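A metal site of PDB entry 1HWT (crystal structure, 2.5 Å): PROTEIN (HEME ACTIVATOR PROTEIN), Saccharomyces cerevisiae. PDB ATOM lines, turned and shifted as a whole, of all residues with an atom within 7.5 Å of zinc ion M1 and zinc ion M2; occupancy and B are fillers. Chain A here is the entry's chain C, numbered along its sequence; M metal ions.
O of Cys 27 is in hydrogen-bond range of OG1 of Thr 31 (3.0 Å). The backbone carbonyl oxygen of Cys 39 is in hydrogen-bond range of a ring nitrogen (ND1) of His 26 (2.9 Å). N of Val 18 lies within hydrogen-bond range of O of Cys 13. O of Cys 20 is in hydrogen-bond range of NZ of Lys 22 (3.2 Å). The side-chain sulfur (SG) of Cys 27 sits close to the backbone NH (N) of Gln 29 (3.7 Å). O of Cys 30 sits at hydrogen-bond distance from N of Val 35 (2.9 Å). OG1 of Thr 33 is in hydrogen-bond range of O of Cys 30.
Of the 27 residues printed, 4 come within 4 Å of zinc ion M1. The nearest printed residue that does not touch zinc ion M1 is Gln 29 (4.4 Å).
Of the 27 residues printed, 4 come within 4 Å of zinc ion M2.
Zinc ion M1 is bound by SG of Cys 27, SG of Cys 13, SG of Cys 20 and SG of Cys 10. Zinc ion M1 has four donor atoms within binding distance.
Zinc ion M2 is bound by SG of Cys 10 (2.3 Å). The side-chain sulfur (SG) of Cys 39 binds zinc ion M2. SG of Cys 30 is bound to zinc ion M2, 2.4 Å away. SG of Cys 27 is bound to zinc ion M2, 2.4 Å away.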
ATOM      1  N   LEU A   8       7.991 -15.461  22.264  1.00  0.00           N
ATOM      2  CA  LEU A   8       7.595 -14.707  23.447  1.00  0.00           C
ATOM      3  C   LEU A   8       6.140 -14.898  23.850  1.00  0.00           C
ATOM      4  O   LEU A   8       5.756 -14.596  24.978  1.00  0.00           O
ATOM      5  CB  LEU A   8       7.863 -13.228  23.220  1.00  0.00           C
ATOM      6  CG  LEU A   8       9.309 -12.917  22.845  1.00  0.00           C
ATOM      7  CD1 LEU A   8       9.451 -11.441  22.553  1.00  0.00           C
ATOM      8  CD2 LEU A   8      10.215 -13.318  23.982  1.00  0.00           C
ATOM      9  N   SER A   9       5.316 -15.385  22.918  1.00  0.00           N
ATOM     10  CA  SER A   9       3.904 -15.611  23.213  1.00  0.00           C
ATOM     11  C   SER A   9       3.732 -17.011  23.760  1.00  0.00           C
ATOM     12  O   SER A   9       4.377 -17.954  23.291  1.00  0.00           O
ATOM     13  CB  SER A   9       3.067 -15.442  21.946  1.00  0.00           C
ATOM     14  OG  SER A   9       3.325 -14.203  21.336  1.00  0.00           O
ATOM     15  N   CYS A  10       2.856 -17.153  24.762  1.00  0.00           N
ATOM     16  CA  CYS A  10       2.588 -18.454  25.359  1.00  0.00           C
ATOM     17  C   CYS A  10       2.133 -19.442  24.278  1.00  0.00           C
ATOM     18  O   CYS A  10       1.507 -19.051  23.303  1.00  0.00           O
ATOM     19  CB  CYS A  10       1.535 -18.334  26.466  1.00  0.00           C
ATOM     20  SG  CYS A  10      -0.197 -18.188  25.915  1.00  0.00           S
ATOM     21  N   THR A  11       2.482 -20.703  24.457  1.00  0.00           N
ATOM     22  CA  THR A  11       2.138 -21.730  23.501  1.00  0.00           C
ATOM     23  C   THR A  11       0.662 -21.768  23.103  1.00  0.00           C
ATOM     24  O   THR A  11       0.341 -21.996  21.948  1.00  0.00           O
ATOM     25  CB  THR A  11       2.551 -23.137  24.008  1.00  0.00           C
ATOM     26  OG1 THR A  11       2.194 -23.285  25.389  1.00  0.00           O
ATOM     27  CG2 THR A  11       4.039 -23.326  23.855  1.00  0.00           C
ATOM     28  N   ILE A  12      -0.242 -21.540  24.054  1.00  0.00           N
ATOM     29  CA  ILE A  12      -1.653 -21.591  23.739  1.00  0.00           C
ATOM     30  C   ILE A  12      -2.086 -20.506  22.773  1.00  0.00           C
ATOM     31  O   ILE A  12      -2.802 -20.779  21.813  1.00  0.00           O
ATOM     32  CB  ILE A  12      -2.531 -21.504  25.003  1.00  0.00           C
ATOM     33  CG1 ILE A  12      -2.267 -22.709  25.912  1.00  0.00           C
ATOM     34  CG2 ILE A  12      -3.997 -21.420  24.623  1.00  0.00           C
ATOM     35  CD1 ILE A  12      -2.521 -24.030  25.253  1.00  0.00           C
ATOM     36  N   CYS A  13      -1.668 -19.265  23.026  1.00  0.00           N
ATOM     37  CA  CYS A  13      -2.025 -18.141  22.154  1.00  0.00           C
ATOM     38  C   CYS A  13      -1.437 -18.370  20.783  1.00  0.00           C
ATOM     39  O   CYS A  13      -2.002 -17.942  19.768  1.00  0.00           O
ATOM     40  CB  CYS A  13      -1.493 -16.829  22.703  1.00  0.00           C
ATOM     41  SG  CYS A  13      -2.524 -16.125  24.021  1.00  0.00           S
ATOM     42  N   ARG A  14      -0.289 -19.019  20.756  1.00  0.00           N
ATOM     43  CA  ARG A  14       0.376 -19.351  19.516  1.00  0.00           C
ATOM     44  C   ARG A  14      -0.558 -20.263  18.729  1.00  0.00           C
ATOM     45  O   ARG A  14      -0.904 -19.961  17.601  1.00  0.00           O
ATOM     46  CB  ARG A  14       1.680 -20.086  19.802  1.00  0.00           C
ATOM     47  CG  ARG A  14       2.880 -19.548  19.050  1.00  0.00           C
ATOM     48  CD  ARG A  14       3.922 -18.988  19.995  1.00  0.00           C
ATOM     49  NE  ARG A  14       4.579 -20.048  20.765  1.00  0.00           N
ATOM     50  CZ  ARG A  14       5.247 -21.078  20.243  1.00  0.00           C
ATOM     51  NH1 ARG A  14       5.353 -21.179  18.921  1.00  0.00           N
ATOM     52  NH2 ARG A  14       5.798 -21.989  21.036  1.00  0.00           N
ATOM     53  N   VAL A  18      -3.906 -15.948  18.414  1.00  0.00           N
ATOM     54  CA  VAL A  18      -4.415 -14.679  18.921  1.00  0.00           C
ATOM     55  C   VAL A  18      -3.255 -13.923  19.536  1.00  0.00           C
ATOM     56  O   VAL A  18      -2.209 -14.494  19.762  1.00  0.00           O
ATOM     57  CB  VAL A  18      -5.489 -14.893  19.985  1.00  0.00           C
ATOM     58  CG1 VAL A  18      -6.667 -15.611  19.373  1.00  0.00           C
ATOM     59  CG2 VAL A  18      -4.942 -15.706  21.115  1.00  0.00           C
ATOM     60  N   LYS A  19      -3.414 -12.644  19.813  1.00  0.00           N
ATOM     61  CA  LYS A  19      -2.343 -11.857  20.392  1.00  0.00           C
ATOM     62  C   LYS A  19      -2.132 -12.156  21.880  1.00  0.00           C
ATOM     63  O   LYS A  19      -3.077 -12.113  22.675  1.00  0.00           O
ATOM     64  CB  LYS A  19      -2.627 -10.368  20.192  1.00  0.00           C
ATOM     65  CG  LYS A  19      -1.847  -9.434  21.105  1.00  0.00           C
ATOM     66  CD  LYS A  19      -0.669  -8.818  20.370  1.00  0.00           C
ATOM     67  CE  LYS A  19      -0.801  -7.292  20.281  1.00  0.00           C
ATOM     68  NZ  LYS A  19      -1.909  -6.844  19.350  1.00  0.00           N
ATOM     69  N   CYS A  20      -0.884 -12.444  22.248  1.00  0.00           N
ATOM     70  CA  CYS A  20      -0.540 -12.728  23.635  1.00  0.00           C
ATOM     71  C   CYS A  20      -0.042 -11.451  24.340  1.00  0.00           C
ATOM     72  O   CYS A  20       0.825 -10.750  23.821  1.00  0.00           O
ATOM     73  CB  CYS A  20       0.550 -13.807  23.702  1.00  0.00           C
ATOM     74  SG  CYS A  20       0.812 -14.493  25.366  1.00  0.00           S
ATOM     75  N   ASP A  21      -0.601 -11.147  25.505  1.00  0.00           N
ATOM     76  CA  ASP A  21      -0.166  -9.968  26.243  1.00  0.00           C
ATOM     77  C   ASP A  21       1.119 -10.255  27.007  1.00  0.00           C
ATOM     78  O   ASP A  21       1.617  -9.401  27.738  1.00  0.00           O
ATOM     79  CB  ASP A  21      -1.234  -9.517  27.220  1.00  0.00           C
ATOM     80  CG  ASP A  21      -1.871 -10.667  27.913  1.00  0.00           C
ATOM     81  OD1 ASP A  21      -2.708 -11.328  27.265  1.00  0.00           O
ATOM     82  OD2 ASP A  21      -1.542 -10.931  29.094  1.00  0.00           O
ATOM     83  N   LYS A  22       1.639 -11.475  26.856  1.00  0.00           N
ATOM     84  CA  LYS A  22       2.882 -11.897  27.492  1.00  0.00           C
ATOM     85  C   LYS A  22       3.022 -11.620  28.978  1.00  0.00           C
ATOM     86  O   LYS A  22       4.137 -11.472  29.485  1.00  0.00           O
ATOM     87  CB  LYS A  22       4.057 -11.271  26.743  1.00  0.00           C
ATOM     88  CG  LYS A  22       4.227 -11.746  25.301  1.00  0.00           C
ATOM     89  CD  LYS A  22       4.164 -10.590  24.308  1.00  0.00           C
ATOM     90  CE  LYS A  22       4.393 -11.069  22.871  1.00  0.00           C
ATOM     91  NZ  LYS A  22       3.418 -10.464  21.886  1.00  0.00           N
ATOM     92  N   LEU A  23       1.903 -11.575  29.688  1.00  0.00           N
ATOM     93  CA  LEU A  23       1.908 -11.323  31.125  1.00  0.00           C
ATOM     94  C   LEU A  23       2.158 -12.608  31.894  1.00  0.00           C
ATOM     95  O   LEU A  23       1.688 -13.663  31.498  1.00  0.00           O
ATOM     96  CB  LEU A  23       0.586 -10.685  31.568  1.00  0.00           C
ATOM     97  CG  LEU A  23       0.207  -9.394  30.806  1.00  0.00           C
ATOM     98  CD1 LEU A  23      -1.097  -8.845  31.390  1.00  0.00           C
ATOM     99  CD2 LEU A  23       1.323  -8.337  30.887  1.00  0.00           C
ATOM    100  N   PRO A  25       2.236 -14.787  35.735  1.00  0.00           N
ATOM    101  CA  PRO A  25       2.744 -16.097  35.322  1.00  0.00           C
ATOM    102  C   PRO A  25       1.999 -16.623  34.111  1.00  0.00           C
ATOM    103  O   PRO A  25       2.536 -17.405  33.321  1.00  0.00           O
ATOM    104  CB  PRO A  25       2.490 -16.968  36.543  1.00  0.00           C
ATOM    105  CG  PRO A  25       1.266 -16.371  37.163  1.00  0.00           C
ATOM    106  CD  PRO A  25       1.404 -14.876  36.944  1.00  0.00           C
ATOM    107  N   HIS A  26       0.757 -16.174  33.970  1.00  0.00           N
ATOM    108  CA  HIS A  26      -0.093 -16.572  32.854  1.00  0.00           C
ATOM    109  C   HIS A  26      -0.715 -15.348  32.234  1.00  0.00           C
ATOM    110  O   HIS A  26      -1.107 -14.419  32.956  1.00  0.00           O
ATOM    111  CB  HIS A  26      -1.209 -17.491  33.338  1.00  0.00           C
ATOM    112  CG  HIS A  26      -0.733 -18.572  34.261  1.00  0.00           C
ATOM    113  ND1 HIS A  26       0.173 -19.527  33.877  1.00  0.00           N
ATOM    114  CD2 HIS A  26      -1.048 -18.846  35.550  1.00  0.00           C
ATOM    115  CE1 HIS A  26       0.411 -20.342  34.886  1.00  0.00           C
ATOM    116  NE2 HIS A  26      -0.325 -19.956  35.908  1.00  0.00           N
ATOM    117  N   CYS A  27      -0.815 -15.350  30.910  1.00  0.00           N
ATOM    118  CA  CYS A  27      -1.374 -14.229  30.166  1.00  0.00           C
ATOM    119  C   CYS A  27      -2.876 -14.133  30.387  1.00  0.00           C
ATOM    120  O   CYS A  27      -3.519 -15.111  30.771  1.00  0.00           O
ATOM    121  CB  CYS A  27      -1.038 -14.364  28.685  1.00  0.00           C
ATOM    122  SG  CYS A  27      -1.992 -15.629  27.805  1.00  0.00           S
ATOM    123  N   GLN A  28      -3.436 -12.945  30.151  1.00  0.00           N
ATOM    124  CA  GLN A  28      -4.870 -12.730  30.345  1.00  0.00           C
ATOM    125  C   GLN A  28      -5.753 -13.454  29.340  1.00  0.00           C
ATOM    126  O   GLN A  28      -6.926 -13.674  29.596  1.00  0.00           O
ATOM    127  CB  GLN A  28      -5.182 -11.235  30.323  1.00  0.00           C
ATOM    128  CG  GLN A  28      -5.086 -10.569  31.675  1.00  0.00           C
ATOM    129  CD  GLN A  28      -6.048 -11.154  32.689  1.00  0.00           C
ATOM    130  OE1 GLN A  28      -5.755 -11.170  33.902  1.00  0.00           O
ATOM    131  NE2 GLN A  28      -7.192 -11.637  32.219  1.00  0.00           N
ATOM    132  N   GLN A  29      -5.207 -13.819  28.185  1.00  0.00           N
ATOM    133  CA  GLN A  29      -5.998 -14.523  27.185  1.00  0.00           C
ATOM    134  C   GLN A  29      -6.357 -15.893  27.713  1.00  0.00           C
ATOM    135  O   GLN A  29      -7.501 -16.309  27.629  1.00  0.00           O
ATOM    136  CB  GLN A  29      -5.204 -14.669  25.893  1.00  0.00           C
ATOM    137  CG  GLN A  29      -5.795 -13.901  24.728  1.00  0.00           C
ATOM    138  CD  GLN A  29      -5.159 -12.543  24.591  1.00  0.00           C
ATOM    139  OE1 GLN A  29      -4.365 -12.141  25.458  1.00  0.00           O
ATOM    140  NE2 GLN A  29      -5.489 -11.838  23.520  1.00  0.00           N
ATOM    141  N   CYS A  30      -5.368 -16.593  28.244  1.00  0.00           N
ATOM    142  CA  CYS A  30      -5.589 -17.909  28.813  1.00  0.00           C
ATOM    143  C   CYS A  30      -6.442 -17.718  30.043  1.00  0.00           C
ATOM    144  O   CYS A  30      -7.379 -18.465  30.287  1.00  0.00           O
ATOM    145  CB  CYS A  30      -4.266 -18.542  29.230  1.00  0.00           C
ATOM    146  SG  CYS A  30      -3.267 -19.249  27.888  1.00  0.00           S
ATOM    147  N   THR A  31      -6.100 -16.710  30.848  1.00  0.00           N
ATOM    148  CA  THR A  31      -6.842 -16.477  32.074  1.00  0.00           C
ATOM    149  C   THR A  31      -8.327 -16.345  31.783  1.00  0.00           C
ATOM    150  O   THR A  31      -9.150 -17.072  32.330  1.00  0.00           O
ATOM    151  CB  THR A  31      -6.366 -15.213  32.775  1.00  0.00           C
ATOM    152  OG1 THR A  31      -5.081 -15.439  33.359  1.00  0.00           O
ATOM    153  CG2 THR A  31      -7.339 -14.813  33.851  1.00  0.00           C
ATOM    154  N   THR A  33     -10.092 -17.235  29.242  1.00  0.00           N
ATOM    155  CA  THR A  33     -10.749 -18.379  28.619  1.00  0.00           C
ATOM    156  C   THR A  33     -10.782 -19.536  29.592  1.00  0.00           C
ATOM    157  O   THR A  33     -11.272 -20.613  29.278  1.00  0.00           O
ATOM    158  CB  THR A  33     -10.041 -18.857  27.324  1.00  0.00           C
ATOM    159  OG1 THR A  33      -8.619 -18.814  27.487  1.00  0.00           O
ATOM    160  CG2 THR A  33     -10.422 -17.966  26.158  1.00  0.00           C
ATOM    161  N   VAL A  35      -8.100 -21.154  30.926  1.00  0.00           N
ATOM    162  CA  VAL A  35      -7.052 -22.145  30.763  1.00  0.00           C
ATOM    163  C   VAL A  35      -5.683 -21.718  31.289  1.00  0.00           C
ATOM    164  O   VAL A  35      -4.655 -22.206  30.822  1.00  0.00           O
ATOM    165  CB  VAL A  35      -6.926 -22.564  29.270  1.00  0.00           C
ATOM    166  CG1 VAL A  35      -8.166 -23.330  28.855  1.00  0.00           C
ATOM    167  CG2 VAL A  35      -6.753 -21.353  28.388  1.00  0.00           C
ATOM    168  N   ALA A  36      -5.680 -20.828  32.275  1.00  0.00           N
ATOM    169  CA  ALA A  36      -4.439 -20.325  32.865  1.00  0.00           C
ATOM    170  C   ALA A  36      -3.518 -21.434  33.326  1.00  0.00           C
ATOM    171  O   ALA A  36      -2.300 -21.301  33.279  1.00  0.00           O
ATOM    172  CB  ALA A  36      -4.748 -19.410  34.024  1.00  0.00           C
ATOM    173  N   LEU A  38      -2.874 -23.930  31.878  1.00  0.00           N
ATOM    174  CA  LEU A  38      -2.218 -24.515  30.722  1.00  0.00           C
ATOM    175  C   LEU A  38      -1.343 -23.480  30.040  1.00  0.00           C
ATOM    176  O   LEU A  38      -0.712 -23.756  29.027  1.00  0.00           O
ATOM    177  CB  LEU A  38      -3.246 -25.033  29.716  1.00  0.00           C
ATOM    178  CG  LEU A  38      -4.252 -26.101  30.155  1.00  0.00           C
ATOM    179  CD1 LEU A  38      -5.042 -26.541  28.944  1.00  0.00           C
ATOM    180  CD2 LEU A  38      -3.539 -27.275  30.795  1.00  0.00           C
ATOM    181  N   CYS A  39      -1.298 -22.291  30.613  1.00  0.00           N
ATOM    182  CA  CYS A  39      -0.506 -21.216  30.024  1.00  0.00           C
ATOM    183  C   CYS A  39       0.924 -21.254  30.481  1.00  0.00           C
ATOM    184  O   CYS A  39       1.198 -21.141  31.667  1.00  0.00           O
ATOM    185  CB  CYS A  39      -1.060 -19.850  30.409  1.00  0.00           C
ATOM    186  SG  CYS A  39      -0.064 -18.510  29.703  1.00  0.00           S
ATOM    187  N   HIS A  40       1.829 -21.421  29.536  1.00  0.00           N
ATOM    188  CA  HIS A  40       3.244 -21.460  29.859  1.00  0.00           C
ATOM    189  C   HIS A  40       4.041 -20.903  28.701  1.00  0.00           C
ATOM    190  O   HIS A  40       3.584 -20.935  27.552  1.00  0.00           O
ATOM    191  CB  HIS A  40       3.682 -22.893  30.197  1.00  0.00           C
ATOM    192  CG  HIS A  40       3.616 -23.848  29.051  1.00  0.00           C
ATOM    193  ND1 HIS A  40       4.676 -24.089  28.210  1.00  0.00           N
ATOM    194  CD2 HIS A  40       2.608 -24.649  28.626  1.00  0.00           C
ATOM    195  CE1 HIS A  40       4.332 -25.006  27.324  1.00  0.00           C
ATOM    196  NE2 HIS A  40       3.083 -25.365  27.552  1.00  0.00           N
ATOM    197  N   TYR A  41       5.218 -20.374  29.015  1.00  0.00           N
ATOM    198  CA  TYR A  41       6.105 -19.798  28.021  1.00  0.00           C
ATOM    199  C   TYR A  41       7.322 -20.670  27.864  1.00  0.00           C
ATOM    200  O   TYR A  41       7.762 -21.323  28.809  1.00  0.00           O
ATOM    201  CB  TYR A  41       6.549 -18.415  28.476  1.00  0.00           C
ATOM    202  CG  TYR A  41       5.406 -17.454  28.655  1.00  0.00           C
ATOM    203  CD1 TYR A  41       4.728 -17.355  29.879  1.00  0.00           C
ATOM    204  CD2 TYR A  41       4.988 -16.638  27.604  1.00  0.00           C
ATOM    205  CE1 TYR A  41       3.648 -16.478  30.034  1.00  0.00           C
ATOM    206  CE2 TYR A  41       3.927 -15.758  27.750  1.00  0.00           C
ATOM    207  CZ  TYR A  41       3.271 -15.677  28.962  1.00  0.00           C
ATOM    208  OH  TYR A  41       2.249 -14.763  29.101  1.00  0.00           O
HETATM  209 ZN    ZN M   1      -1.038 -15.955  25.764  1.00  0.00          ZN
HETATM  210 ZN    ZN M   2      -1.312 -17.919  27.862  1.00  0.00          ZN
